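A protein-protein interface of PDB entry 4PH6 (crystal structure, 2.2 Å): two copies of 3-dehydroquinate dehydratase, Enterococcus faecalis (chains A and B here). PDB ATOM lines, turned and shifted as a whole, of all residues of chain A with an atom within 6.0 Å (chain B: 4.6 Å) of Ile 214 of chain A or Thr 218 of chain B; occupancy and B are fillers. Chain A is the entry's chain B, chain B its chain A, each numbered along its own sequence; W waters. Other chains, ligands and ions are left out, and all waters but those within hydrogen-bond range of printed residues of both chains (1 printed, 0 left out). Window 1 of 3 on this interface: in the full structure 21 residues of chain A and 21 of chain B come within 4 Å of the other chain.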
ATOM      1  N   VAL A 184     -15.680  24.984  -6.487  1.00  0.00           N
ATOM      2  CA  VAL A 184     -15.758  25.240  -7.920  1.00  0.00           C
ATOM      3  C   VAL A 184     -14.719  26.290  -8.307  1.00  0.00           C
ATOM      4  O   VAL A 184     -14.001  26.132  -9.291  1.00  0.00           O
ATOM      5  CB  VAL A 184     -17.166  25.722  -8.350  1.00  0.00           C
ATOM      6  CG1 VAL A 184     -17.247  25.843  -9.871  1.00  0.00           C
ATOM      7  CG2 VAL A 184     -18.234  24.772  -7.818  1.00  0.00           C
ATOM      8  N   LEU A 188     -11.635  26.215 -10.911  1.00  0.00           N
ATOM      9  CA  LEU A 188     -11.494  27.242 -11.940  1.00  0.00           C
ATOM     10  C   LEU A 188     -10.150  27.964 -11.792  1.00  0.00           C
ATOM     11  O   LEU A 188      -9.458  28.175 -12.782  1.00  0.00           O
ATOM     12  CB  LEU A 188     -12.661  28.235 -11.882  1.00  0.00           C
ATOM     13  CG  LEU A 188     -14.051  27.680 -12.233  1.00  0.00           C
ATOM     14  CD1 LEU A 188     -15.128  28.702 -11.965  1.00  0.00           C
ATOM     15  CD2 LEU A 188     -14.122  27.229 -13.702  1.00  0.00           C
ATOM     16  N   GLN A 210     -23.992  19.525 -10.427  1.00  0.00           N
ATOM     17  CA  GLN A 210     -24.751  20.738 -10.688  1.00  0.00           C
ATOM     18  C   GLN A 210     -23.989  21.989 -10.259  1.00  0.00           C
ATOM     19  O   GLN A 210     -24.014  23.001 -10.971  1.00  0.00           O
ATOM     20  CB  GLN A 210     -26.111  20.670  -9.985  1.00  0.00           C
ATOM     21  CG  GLN A 210     -27.069  21.774 -10.413  1.00  0.00           C
ATOM     22  CD  GLN A 210     -27.418  21.688 -11.886  1.00  0.00           C
ATOM     23  OE1 GLN A 210     -27.599  20.599 -12.432  1.00  0.00           O
ATOM     24  NE2 GLN A 210     -27.513  22.842 -12.541  1.00  0.00           N
ATOM     25  N   LEU A 211     -23.304  21.912  -9.113  1.00  0.00           N
ATOM     26  CA  LEU A 211     -22.508  23.037  -8.604  1.00  0.00           C
ATOM     27  C   LEU A 211     -21.431  23.524  -9.584  1.00  0.00           C
ATOM     28  O   LEU A 211     -21.241  24.729  -9.749  1.00  0.00           O
ATOM     29  CB  LEU A 211     -21.831  22.670  -7.275  1.00  0.00           C
ATOM     30  CG  LEU A 211     -22.671  22.567  -6.000  1.00  0.00           C
ATOM     31  CD1 LEU A 211     -21.832  22.138  -4.814  1.00  0.00           C
ATOM     32  CD2 LEU A 211     -23.361  23.874  -5.711  1.00  0.00           C
ATOM     33  N   GLY A 212     -20.725  22.588 -10.221  1.00  0.00           N
ATOM     34  CA  GLY A 212     -19.601  22.935 -11.070  1.00  0.00           C
ATOM     35  C   GLY A 212     -19.936  23.057 -12.547  1.00  0.00           C
ATOM     36  O   GLY A 212     -19.037  23.116 -13.391  1.00  0.00           O
ATOM     37  N   MET A 213     -21.229  23.095 -12.865  1.00  0.00           N
ATOM     38  CA  MET A 213     -21.683  23.144 -14.259  1.00  0.00           C
ATOM     39  C   MET A 213     -21.066  24.296 -15.076  1.00  0.00           C
ATOM     40  O   MET A 213     -20.774  24.137 -16.265  1.00  0.00           O
ATOM     41  CB  MET A 213     -23.212  23.235 -14.293  1.00  0.00           C
ATOM     42  CG  MET A 213     -23.817  23.095 -15.671  1.00  0.00           C
ATOM     43  SD  MET A 213     -25.606  22.856 -15.615  1.00  0.00           S
ATOM     44  CE  MET A 213     -25.685  21.231 -14.876  1.00  0.00           C
ATOM     45  N   ILE A 214     -20.854  25.444 -14.436  1.00  0.00           N
ATOM     46  CA  ILE A 214     -20.221  26.586 -15.095  1.00  0.00           C
ATOM     47  C   ILE A 214     -18.841  26.296 -15.674  1.00  0.00           C
ATOM     48  O   ILE A 214     -18.439  26.935 -16.636  1.00  0.00           O
ATOM     49  CB  ILE A 214     -20.042  27.769 -14.141  1.00  0.00           C
ATOM     50  CG1 ILE A 214     -19.311  27.309 -12.879  1.00  0.00           C
ATOM     51  CG2 ILE A 214     -21.374  28.389 -13.829  1.00  0.00           C
ATOM     52  CD1 ILE A 214     -18.963  28.418 -11.945  1.00  0.00           C
ATOM     53  N   SER A 215     -18.109  25.361 -15.076  1.00  0.00           N
ATOM     54  CA  SER A 215     -16.758  25.068 -15.532  1.00  0.00           C
ATOM     55  C   SER A 215     -16.784  24.327 -16.866  1.00  0.00           C
ATOM     56  O   SER A 215     -15.742  24.112 -17.475  1.00  0.00           O
ATOM     57  CB  SER A 215     -15.990  24.245 -14.488  1.00  0.00           C
ATOM     58  OG  SER A 215     -16.465  22.912 -14.406  1.00  0.00           O
ATOM     59  N   ARG A 216     -17.982  23.938 -17.306  1.00  0.00           N
ATOM     60  CA  ARG A 216     -18.154  23.241 -18.572  1.00  0.00           C
ATOM     61  C   ARG A 216     -18.348  24.202 -19.735  1.00  0.00           C
ATOM     62  O   ARG A 216     -18.247  23.792 -20.889  1.00  0.00           O
ATOM     63  CB  ARG A 216     -19.340  22.278 -18.509  1.00  0.00           C
ATOM     64  CG  ARG A 216     -19.232  21.222 -17.426  1.00  0.00           C
ATOM     65  CD  ARG A 216     -20.271  20.121 -17.624  1.00  0.00           C
ATOM     66  NE  ARG A 216     -20.144  19.070 -16.623  1.00  0.00           N
ATOM     67  CZ  ARG A 216     -19.275  18.066 -16.696  1.00  0.00           C
ATOM     68  NH1 ARG A 216     -18.458  17.962 -17.737  1.00  0.00           N
ATOM     69  NH2 ARG A 216     -19.226  17.156 -15.732  1.00  0.00           N
ATOM     70  N   VAL A 217     -18.618  25.477 -19.436  1.00  0.00           N
ATOM     71  CA  VAL A 217     -18.789  26.478 -20.489  1.00  0.00           C
ATOM     72  C   VAL A 217     -17.739  27.603 -20.417  1.00  0.00           C
ATOM     73  O   VAL A 217     -17.755  28.529 -21.219  1.00  0.00           O
ATOM     74  CB  VAL A 217     -20.209  27.096 -20.446  1.00  0.00           C
ATOM     75  CG1 VAL A 217     -21.263  26.009 -20.584  1.00  0.00           C
ATOM     76  CG2 VAL A 217     -20.429  27.909 -19.147  1.00  0.00           C
ATOM     77  N   THR A 218     -16.807  27.511 -19.478  1.00  0.00           N
ATOM     78  CA  THR A 218     -15.851  28.597 -19.283  1.00  0.00           C
ATOM     79  C   THR A 218     -14.432  28.250 -19.724  1.00  0.00           C
ATOM     80  O   THR A 218     -13.472  28.924 -19.328  1.00  0.00           O
ATOM     81  CB  THR A 218     -15.816  29.030 -17.806  1.00  0.00           C
ATOM     82  OG1 THR A 218     -15.585  27.887 -16.966  1.00  0.00           O
ATOM     83  CG2 THR A 218     -17.127  29.621 -17.432  1.00  0.00           C
ATOM     84  N   GLY A 219     -14.303  27.217 -20.559  1.00  0.00           N
ATOM     85  CA  GLY A 219     -13.009  26.723 -20.993  1.00  0.00           C
ATOM     86  C   GLY A 219     -12.172  27.769 -21.696  1.00  0.00           C
ATOM     87  O   GLY A 219     -10.963  27.874 -21.450  1.00  0.00           O
ATOM     88  N   LEU B 188     -15.394  36.931  -8.566  1.00  0.00           N
ATOM     89  CA  LEU B 188     -16.228  35.800  -8.151  1.00  0.00           C
ATOM     90  C   LEU B 188     -15.897  35.339  -6.724  1.00  0.00           C
ATOM     91  O   LEU B 188     -16.798  35.097  -5.932  1.00  0.00           O
ATOM     92  CB  LEU B 188     -16.090  34.635  -9.136  1.00  0.00           C
ATOM     93  CG  LEU B 188     -16.666  34.889 -10.530  1.00  0.00           C
ATOM     94  CD1 LEU B 188     -16.357  33.756 -11.488  1.00  0.00           C
ATOM     95  CD2 LEU B 188     -18.164  35.100 -10.427  1.00  0.00           C
ATOM     96  N   ILE B 214     -19.750  35.553 -17.381  1.00  0.00           N
ATOM     97  CA  ILE B 214     -20.124  34.471 -16.472  1.00  0.00           C
ATOM     98  C   ILE B 214     -20.598  34.943 -15.094  1.00  0.00           C
ATOM     99  O   ILE B 214     -21.377  34.259 -14.446  1.00  0.00           O
ATOM    100  CB  ILE B 214     -18.958  33.509 -16.233  1.00  0.00           C
ATOM    101  CG1 ILE B 214     -17.726  34.302 -15.793  1.00  0.00           C
ATOM    102  CG2 ILE B 214     -18.688  32.717 -17.477  1.00  0.00           C
ATOM    103  CD1 ILE B 214     -16.639  33.470 -15.185  1.00  0.00           C
ATOM    104  N   SER B 215     -20.113  36.093 -14.642  1.00  0.00           N
ATOM    105  CA  SER B 215     -20.511  36.619 -13.335  1.00  0.00           C
ATOM    106  C   SER B 215     -21.969  37.068 -13.345  1.00  0.00           C
ATOM    107  O   SER B 215     -22.549  37.337 -12.302  1.00  0.00           O
ATOM    108  CB  SER B 215     -19.606  37.788 -12.918  1.00  0.00           C
ATOM    109  OG  SER B 215     -19.841  38.950 -13.702  1.00  0.00           O
ATOM    110  N   ARG B 216     -22.562  37.153 -14.532  1.00  0.00           N
ATOM    111  CA  ARG B 216     -23.928  37.634 -14.635  1.00  0.00           C
ATOM    112  C   ARG B 216     -24.940  36.496 -14.562  1.00  0.00           C
ATOM    113  O   ARG B 216     -26.129  36.751 -14.441  1.00  0.00           O
ATOM    114  CB  ARG B 216     -24.127  38.421 -15.926  1.00  0.00           C
ATOM    115  CG  ARG B 216     -23.222  39.636 -16.063  1.00  0.00           C
ATOM    116  CD  ARG B 216     -23.675  40.519 -17.206  1.00  0.00           C
ATOM    117  NE  ARG B 216     -22.825  41.689 -17.412  1.00  0.00           N
ATOM    118  CZ  ARG B 216     -22.967  42.852 -16.784  1.00  0.00           C
ATOM    119  NH1 ARG B 216     -23.918  43.017 -15.872  1.00  0.00           N
ATOM    120  NH2 ARG B 216     -22.139  43.855 -17.058  1.00  0.00           N
ATOM    121  N   VAL B 217     -24.471  35.246 -14.615  1.00  0.00           N
ATOM    122  CA  VAL B 217     -25.384  34.112 -14.567  1.00  0.00           C
ATOM    123  C   VAL B 217     -25.120  33.151 -13.404  1.00  0.00           C
ATOM    124  O   VAL B 217     -25.876  32.188 -13.197  1.00  0.00           O
ATOM    125  CB  VAL B 217     -25.340  33.321 -15.892  1.00  0.00           C
ATOM    126  CG1 VAL B 217     -25.591  34.265 -17.074  1.00  0.00           C
ATOM    127  CG2 VAL B 217     -24.005  32.582 -16.043  1.00  0.00           C
ATOM    128  N   THR B 218     -24.063  33.429 -12.643  1.00  0.00           N
ATOM    129  CA  THR B 218     -23.641  32.568 -11.543  1.00  0.00           C
ATOM    130  C   THR B 218     -24.076  33.063 -10.179  1.00  0.00           C
ATOM    131  O   THR B 218     -23.620  32.531  -9.171  1.00  0.00           O
ATOM    132  CB  THR B 218     -22.093  32.410 -11.503  1.00  0.00           C
ATOM    133  OG1 THR B 218     -21.457  33.704 -11.479  1.00  0.00           O
ATOM    134  CG2 THR B 218     -21.619  31.643 -12.701  1.00  0.00           C
ATOM    135  N   GLY B 219     -24.932  34.086 -10.144  1.00  0.00           N
ATOM    136  CA  GLY B 219     -25.360  34.701  -8.899  1.00  0.00           C
ATOM    137  C   GLY B 219     -25.825  33.703  -7.851  1.00  0.00           C
ATOM    138  O   GLY B 219     -25.472  33.816  -6.683  1.00  0.00           O
ATOM    139  N   GLN B 220     -26.610  32.712  -8.247  1.00  0.00           N
ATOM    140  CA  GLN B 220     -27.105  31.755  -7.261  1.00  0.00           C
ATOM    141  C   GLN B 220     -25.952  30.973  -6.616  1.00  0.00           C
ATOM    142  O   GLN B 220     -25.958  30.708  -5.419  1.00  0.00           O
ATOM    143  CB  GLN B 220     -28.104  30.775  -7.877  1.00  0.00           C
ATOM    144  CG  GLN B 220     -28.819  29.946  -6.807  1.00  0.00           C
ATOM    145  CD  GLN B 220     -29.664  28.819  -7.358  1.00  0.00           C
ATOM    146  OE1 GLN B 220     -29.412  28.305  -8.451  1.00  0.00           O
ATOM    147  NE2 GLN B 220     -30.678  28.425  -6.603  1.00  0.00           N
ATOM    148  N   LEU B 221     -24.958  30.621  -7.409  1.00  0.00           N
ATOM    149  CA  LEU B 221     -23.852  29.831  -6.896  1.00  0.00           C
ATOM    150  C   LEU B 221     -22.985  30.600  -5.905  1.00  0.00           C
ATOM    151  O   LEU B 221     -22.617  30.065  -4.855  1.00  0.00           O
ATOM    152  CB  LEU B 221     -22.988  29.331  -8.052  1.00  0.00           C
ATOM    153  CG  LEU B 221     -21.763  28.504  -7.677  1.00  0.00           C
ATOM    154  CD1 LEU B 221     -22.173  27.313  -6.824  1.00  0.00           C
ATOM    155  CD2 LEU B 221     -21.058  28.044  -8.943  1.00  0.00           C
ATOM    156  N   PHE B 222     -22.658  31.847  -6.233  1.00  0.00           N
ATOM    157  CA  PHE B 222     -21.656  32.582  -5.471  1.00  0.00           C
ATOM    158  C   PHE B 222     -22.264  33.641  -4.545  1.00  0.00           C
ATOM    159  O   PHE B 222     -21.567  34.201  -3.710  1.00  0.00           O
ATOM    160  CB  PHE B 222     -20.638  33.232  -6.414  1.00  0.00           C
ATOM    161  CG  PHE B 222     -19.879  32.250  -7.257  1.00  0.00           C
ATOM    162  CD1 PHE B 222     -19.924  32.322  -8.633  1.00  0.00           C
ATOM    163  CD2 PHE B 222     -19.121  31.251  -6.673  1.00  0.00           C
ATOM    164  CE1 PHE B 222     -19.214  31.408  -9.426  1.00  0.00           C
ATOM    165  CE2 PHE B 222     -18.420  30.341  -7.450  1.00  0.00           C
ATOM    166  CZ  PHE B 222     -18.465  30.418  -8.828  1.00  0.00           C
ATOM    167  N   PHE B 252     -28.178  27.029 -14.914  1.00  0.00           N
ATOM    168  CA  PHE B 252     -27.174  26.922 -13.864  1.00  0.00           C
ATOM    169  C   PHE B 252     -27.791  26.976 -12.469  1.00  0.00           C
ATOM    170  O   PHE B 252     -27.087  27.188 -11.489  1.00  0.00           O
ATOM    171  CB  PHE B 252     -26.114  28.009 -14.022  1.00  0.00           C
ATOM    172  CG  PHE B 252     -25.291  27.869 -15.275  1.00  0.00           C
ATOM    173  CD1 PHE B 252     -24.504  26.746 -15.477  1.00  0.00           C
ATOM    174  CD2 PHE B 252     -25.298  28.859 -16.248  1.00  0.00           C
ATOM    175  CE1 PHE B 252     -23.745  26.604 -16.629  1.00  0.00           C
ATOM    176  CE2 PHE B 252     -24.534  28.720 -17.411  1.00  0.00           C
ATOM    177  CZ  PHE B 252     -23.758  27.595 -17.597  1.00  0.00           C
HETATM  178  O   HOH W   1     -24.651  25.269 -11.867  1.00  0.00           O
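The backbone carbonyl oxygen of Ile 214 of chain B sits at hydrogen-bond distance from the side-chain hydroxyl of Thr 218 of chain B (3.0 Å). SD of Met 213 of chain A sits close to NE2 of Gln 210 of chain A (3.6 Å). The side-chain hydroxyl (OG1) of Thr 218 of chain A is in hydrogen-bond range of the backbone carbonyl oxygen (O) of Ile 214 of chain A.
Among the printed residues, merely in contact across the chains: Leu 211 of chain A with Leu 221 of chain B, Met 213 of chain A with Phe 252 of chain B, Ile 214 of chain A with Thr 218 of chain B, Ile 214 of chain A with Leu 221 of chain B, Ile 214 of chain A with Phe 222 of chain B, Ile 214 of chain A with Phe 252 of chain B, Val 217 of chain A with Phe 252 of chain B and Thr 218 of chain A with Ile 214 of chain B.
Ile 214 of chain A touches Thr 218 of chain B, and with the chains exchanged Thr 218 of chain A touches Ile 214 of chain B. Positions printed for both chains: 188, 214, 215, 216, 217, 218 and 219.
Water W1 lies within hydrogen-bond range of the backbone carbonyl oxygen (O) of Gln 210 of chain A (2.5 Å) and the backbone carbonyl oxygen (O) of Phe 252 of chain B (3.1 Å).
Of the printed residues of chain B, Leu 211 of chain A touches Leu 221 (3.4 Å). Of chain B, only Thr 218, Leu 221, Phe 222 and Phe 252 come within 4 Å of Ile 214 of chain A. Printed residues of chain A within 4 Å of Ile 214 of chain B: Thr 218 (3.5 Å). Of chain A, only Ile 214 (3.5 Å) comes within 4 Å of Thr 218 of chain B. Of the printed residues of chain A, Leu 221 of chain B touches Leu 211 (3.4 Å) and Ile 214 (3.7 Å). The nearest printed residue of chain B that does not touch Met 213 of chain A is Leu 221 of chain B (6.3 Å).
Printed residues of chain B that touch a printed residue of chain A: Ile 214, Thr 218, Leu 221, Phe 222 and Phe 252. Hydrophobic or aromatic side chains of chain B that line the printed part of chain A: Ile 214, Leu 221, Phe 222 and Phe 252. Along chain B the printed residues that touch a printed residue of chain A span positions 214 to 252. Printed residues of chain A that touch a printed residue of chain B: Leu 211, Met 213, Ile 214, Val 217 and Thr 218. Hydrophobic or aromatic side chains of chain A that line the printed part of chain B: Leu 211, Met 213, Ile 214 and Val 217.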
